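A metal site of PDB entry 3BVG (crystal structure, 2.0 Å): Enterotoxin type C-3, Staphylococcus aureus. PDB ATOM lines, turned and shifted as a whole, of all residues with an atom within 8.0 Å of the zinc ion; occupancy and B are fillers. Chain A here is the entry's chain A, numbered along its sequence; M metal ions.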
ATOM      1  N   ALA A  35     -25.533 -22.452 -19.488  1.00  0.00           N
ATOM      2  CA  ALA A  35     -25.333 -22.276 -20.911  1.00  0.00           C
ATOM      3  C   ALA A  35     -24.148 -23.076 -21.382  1.00  0.00           C
ATOM      4  O   ALA A  35     -23.286 -23.429 -20.606  1.00  0.00           O
ATOM      5  CB  ALA A  35     -25.204 -20.801 -21.276  1.00  0.00           C
ATOM      6  N   THR A  36     -24.116 -23.379 -22.682  1.00  0.00           N
ATOM      7  CA  THR A  36     -23.197 -24.394 -23.202  1.00  0.00           C
ATOM      8  C   THR A  36     -22.559 -23.893 -24.533  1.00  0.00           C
ATOM      9  O   THR A  36     -23.269 -23.442 -25.386  1.00  0.00           O
ATOM     10  CB  THR A  36     -24.031 -25.717 -23.396  1.00  0.00           C
ATOM     11  OG1 THR A  36     -23.839 -26.605 -22.259  1.00  0.00           O
ATOM     12  CG2 THR A  36     -23.723 -26.393 -24.697  1.00  0.00           C
ATOM     13  N   LYS A  37     -21.224 -24.003 -24.640  1.00  0.00           N
ATOM     14  CA  LYS A  37     -20.424 -23.602 -25.807  1.00  0.00           C
ATOM     15  C   LYS A  37     -20.772 -22.163 -26.254  1.00  0.00           C
ATOM     16  O   LYS A  37     -21.235 -21.930 -27.386  1.00  0.00           O
ATOM     17  CB  LYS A  37     -20.541 -24.621 -26.964  1.00  0.00           C
ATOM     18  CG  LYS A  37     -20.292 -26.060 -26.586  1.00  0.00           C
ATOM     19  CD  LYS A  37     -20.815 -27.005 -27.638  1.00  0.00           C
ATOM     20  CE  LYS A  37     -20.061 -26.788 -28.983  1.00  0.00           C
ATOM     21  NZ  LYS A  37     -20.498 -27.855 -29.946  1.00  0.00           N
ATOM     22  N   VAL A  38     -20.586 -21.215 -25.340  1.00  0.00           N
ATOM     23  CA  VAL A  38     -20.847 -19.796 -25.572  1.00  0.00           C
ATOM     24  C   VAL A  38     -19.546 -19.037 -25.468  1.00  0.00           C
ATOM     25  O   VAL A  38     -18.573 -19.528 -24.889  1.00  0.00           O
ATOM     26  CB  VAL A  38     -21.907 -19.204 -24.567  1.00  0.00           C
ATOM     27  CG1 VAL A  38     -23.315 -19.839 -24.777  1.00  0.00           C
ATOM     28  CG2 VAL A  38     -21.437 -19.289 -23.090  1.00  0.00           C
ATOM     29  N   VAL A  81     -14.393 -20.563 -25.867  1.00  0.00           N
ATOM     30  CA  VAL A  81     -15.657 -21.290 -25.881  1.00  0.00           C
ATOM     31  C   VAL A  81     -15.863 -22.037 -24.543  1.00  0.00           C
ATOM     32  O   VAL A  81     -15.120 -22.961 -24.205  1.00  0.00           O
ATOM     33  CB  VAL A  81     -15.769 -22.201 -27.136  1.00  0.00           C
ATOM     34  CG1 VAL A  81     -17.130 -22.874 -27.161  1.00  0.00           C
ATOM     35  CG2 VAL A  81     -15.591 -21.338 -28.432  1.00  0.00           C
ATOM     36  N   VAL A  82     -16.862 -21.594 -23.789  1.00  0.00           N
ATOM     37  CA  VAL A  82     -17.054 -21.970 -22.410  1.00  0.00           C
ATOM     38  C   VAL A  82     -18.468 -22.558 -22.167  1.00  0.00           C
ATOM     39  O   VAL A  82     -19.380 -22.359 -22.983  1.00  0.00           O
ATOM     40  CB  VAL A  82     -16.765 -20.764 -21.402  1.00  0.00           C
ATOM     41  CG1 VAL A  82     -15.278 -20.226 -21.494  1.00  0.00           C
ATOM     42  CG2 VAL A  82     -17.799 -19.614 -21.510  1.00  0.00           C
ATOM     43  N   ASP A  83     -18.587 -23.328 -21.080  1.00  0.00           N
ATOM     44  CA  ASP A  83     -19.886 -23.656 -20.481  1.00  0.00           C
ATOM     45  C   ASP A  83     -20.032 -22.833 -19.199  1.00  0.00           C
ATOM     46  O   ASP A  83     -18.998 -22.493 -18.603  1.00  0.00           O
ATOM     47  CB  ASP A  83     -20.021 -25.164 -20.210  1.00  0.00           C
ATOM     48  CG  ASP A  83     -19.664 -26.000 -21.438  1.00  0.00           C
ATOM     49  OD1 ASP A  83     -20.008 -25.622 -22.582  1.00  0.00           O
ATOM     50  OD2 ASP A  83     -18.935 -26.975 -21.251  1.00  0.00           O
ATOM     51  N   VAL A  84     -21.276 -22.516 -18.810  1.00  0.00           N
ATOM     52  CA  VAL A  84     -21.543 -21.568 -17.738  1.00  0.00           C
ATOM     53  C   VAL A  84     -22.546 -22.245 -16.845  1.00  0.00           C
ATOM     54  O   VAL A  84     -23.529 -22.805 -17.316  1.00  0.00           O
ATOM     55  CB  VAL A  84     -22.111 -20.198 -18.191  1.00  0.00           C
ATOM     56  CG1 VAL A  84     -22.352 -19.285 -16.943  1.00  0.00           C
ATOM     57  CG2 VAL A  84     -21.194 -19.513 -19.147  1.00  0.00           C
ATOM     58  N   THR A 114     -16.114 -22.640 -17.222  1.00  0.00           N
ATOM     59  CA  THR A 114     -15.131 -23.679 -17.533  1.00  0.00           C
ATOM     60  C   THR A 114     -14.994 -23.741 -19.052  1.00  0.00           C
ATOM     61  O   THR A 114     -15.978 -23.570 -19.773  1.00  0.00           O
ATOM     62  CB  THR A 114     -15.596 -25.067 -17.023  1.00  0.00           C
ATOM     63  OG1 THR A 114     -16.964 -25.270 -17.396  1.00  0.00           O
ATOM     64  CG2 THR A 114     -15.479 -25.189 -15.446  1.00  0.00           C
ATOM     65  N   LYS A 115     -13.783 -23.963 -19.549  1.00  0.00           N
ATOM     66  CA  LYS A 115     -13.587 -24.243 -20.988  1.00  0.00           C
ATOM     67  C   LYS A 115     -14.391 -25.493 -21.379  1.00  0.00           C
ATOM     68  O   LYS A 115     -14.530 -26.419 -20.611  1.00  0.00           O
ATOM     69  CB  LYS A 115     -12.096 -24.423 -21.343  1.00  0.00           C
ATOM     70  CG  LYS A 115     -11.178 -23.190 -21.156  1.00  0.00           C
ATOM     71  CD  LYS A 115      -9.750 -23.710 -20.695  1.00  0.00           C
ATOM     72  CE  LYS A 115      -8.594 -22.674 -20.686  1.00  0.00           C
ATOM     73  NZ  LYS A 115      -7.424 -23.263 -19.875  1.00  0.00           N
ATOM     74  N   HIS A 116     -14.993 -25.451 -22.556  1.00  0.00           N
ATOM     75  CA  HIS A 116     -15.782 -26.587 -23.112  1.00  0.00           C
ATOM     76  C   HIS A 116     -14.867 -27.701 -23.601  1.00  0.00           C
ATOM     77  O   HIS A 116     -15.071 -28.885 -23.315  1.00  0.00           O
ATOM     78  CB  HIS A 116     -16.592 -26.050 -24.315  1.00  0.00           C
ATOM     79  CG  HIS A 116     -17.147 -27.125 -25.204  1.00  0.00           C
ATOM     80  ND1 HIS A 116     -18.128 -28.001 -24.793  1.00  0.00           N
ATOM     81  CD2 HIS A 116     -16.854 -27.449 -26.486  1.00  0.00           C
ATOM     82  CE1 HIS A 116     -18.389 -28.857 -25.776  1.00  0.00           C
ATOM     83  NE2 HIS A 116     -17.669 -28.508 -26.829  1.00  0.00           N
ATOM     84  N   GLU A 117     -13.859 -27.302 -24.387  1.00  0.00           N
ATOM     85  CA  GLU A 117     -13.083 -28.269 -25.165  1.00  0.00           C
ATOM     86  C   GLU A 117     -12.286 -29.147 -24.224  1.00  0.00           C
ATOM     87  O   GLU A 117     -11.579 -28.628 -23.345  1.00  0.00           O
ATOM     88  CB  GLU A 117     -12.144 -27.577 -26.169  1.00  0.00           C
ATOM     89  CG  GLU A 117     -12.806 -26.637 -27.236  1.00  0.00           C
ATOM     90  CD  GLU A 117     -13.741 -27.373 -28.254  1.00  0.00           C
ATOM     91  OE1 GLU A 117     -13.449 -28.560 -28.641  1.00  0.00           O
ATOM     92  OE2 GLU A 117     -14.755 -26.732 -28.651  1.00  0.00           O
ATOM     93  N   GLY A 118     -12.417 -30.457 -24.387  1.00  0.00           N
ATOM     94  CA  GLY A 118     -11.690 -31.400 -23.510  1.00  0.00           C
ATOM     95  C   GLY A 118     -12.272 -31.702 -22.134  1.00  0.00           C
ATOM     96  O   GLY A 118     -11.662 -32.467 -21.347  1.00  0.00           O
ATOM     97  N   ASN A 119     -13.419 -31.122 -21.822  1.00  0.00           N
ATOM     98  CA  ASN A 119     -13.950 -31.098 -20.429  1.00  0.00           C
ATOM     99  C   ASN A 119     -15.078 -32.037 -20.123  1.00  0.00           C
ATOM    100  O   ASN A 119     -15.744 -31.906 -19.091  1.00  0.00           O
ATOM    101  CB  ASN A 119     -14.329 -29.676 -19.922  1.00  0.00           C
ATOM    102  CG  ASN A 119     -14.284 -29.592 -18.376  1.00  0.00           C
ATOM    103  OD1 ASN A 119     -13.453 -30.206 -17.756  1.00  0.00           O
ATOM    104  ND2 ASN A 119     -15.199 -28.855 -17.780  1.00  0.00           N
ATOM    105  N   HIS A 120     -15.291 -33.005 -20.994  1.00  0.00           N
ATOM    106  CA  HIS A 120     -16.442 -33.881 -20.810  1.00  0.00           C
ATOM    107  C   HIS A 120     -16.003 -35.335 -20.861  1.00  0.00           C
ATOM    108  O   HIS A 120     -14.957 -35.674 -21.444  1.00  0.00           O
ATOM    109  CB  HIS A 120     -17.534 -33.538 -21.843  1.00  0.00           C
ATOM    110  CG  HIS A 120     -18.128 -32.166 -21.678  1.00  0.00           C
ATOM    111  ND1 HIS A 120     -18.962 -31.831 -20.629  1.00  0.00           N
ATOM    112  CD2 HIS A 120     -17.985 -31.037 -22.414  1.00  0.00           C
ATOM    113  CE1 HIS A 120     -19.332 -30.569 -20.752  1.00  0.00           C
ATOM    114  NE2 HIS A 120     -18.734 -30.062 -21.803  1.00  0.00           N
ATOM    115  N   ASP A 148     -21.634 -33.459 -15.956  1.00  0.00           N
ATOM    116  CA  ASP A 148     -20.931 -34.076 -17.075  1.00  0.00           C
ATOM    117  C   ASP A 148     -19.545 -33.453 -17.282  1.00  0.00           C
ATOM    118  O   ASP A 148     -18.874 -33.717 -18.273  1.00  0.00           O
ATOM    119  CB  ASP A 148     -21.812 -34.024 -18.348  1.00  0.00           C
ATOM    120  CG  ASP A 148     -22.048 -32.625 -18.821  1.00  0.00           C
ATOM    121  OD1 ASP A 148     -21.510 -31.704 -18.211  1.00  0.00           O
ATOM    122  OD2 ASP A 148     -22.802 -32.444 -19.774  1.00  0.00           O
ATOM    123  N   LYS A 149     -19.069 -32.648 -16.317  1.00  0.00           N
ATOM    124  CA  LYS A 149     -17.813 -31.945 -16.528  1.00  0.00           C
ATOM    125  C   LYS A 149     -16.693 -32.600 -15.794  1.00  0.00           C
ATOM    126  O   LYS A 149     -16.889 -33.097 -14.685  1.00  0.00           O
ATOM    127  CB  LYS A 149     -17.873 -30.494 -16.082  1.00  0.00           C
ATOM    128  CG  LYS A 149     -18.722 -29.564 -16.935  1.00  0.00           C
ATOM    129  CD  LYS A 149     -18.995 -28.291 -16.144  1.00  0.00           C
ATOM    130  CE  LYS A 149     -19.869 -27.336 -17.043  1.00  0.00           C
ATOM    131  NZ  LYS A 149     -21.273 -27.519 -16.674  1.00  0.00           N
HETATM  132 ZN    ZN M   1     -19.186 -28.383 -22.827  1.00  0.00          ZN
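The side-chain carboxylate of Asp 83 is in hydrogen-bond range of the backbone NH of Lys 37. N of Asp 83 sits at hydrogen-bond distance from O of Thr 114. N of His 116 sits at hydrogen-bond distance from O of Val 81 (3.0 Å). A ring nitrogen (ND1) of His 120 sits at hydrogen-bond distance from the backbone carbonyl oxygen of Asp 148.
The nearest printed residue that does not touch the zinc ion is Lys 37 (4.6 Å).
The zinc ion is bound by a ring nitrogen (NE2) of His 120, the side-chain carboxylate of Asp 83 and a ring nitrogen (ND1) of His 116. The zinc ion has three donor atoms within binding distance.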
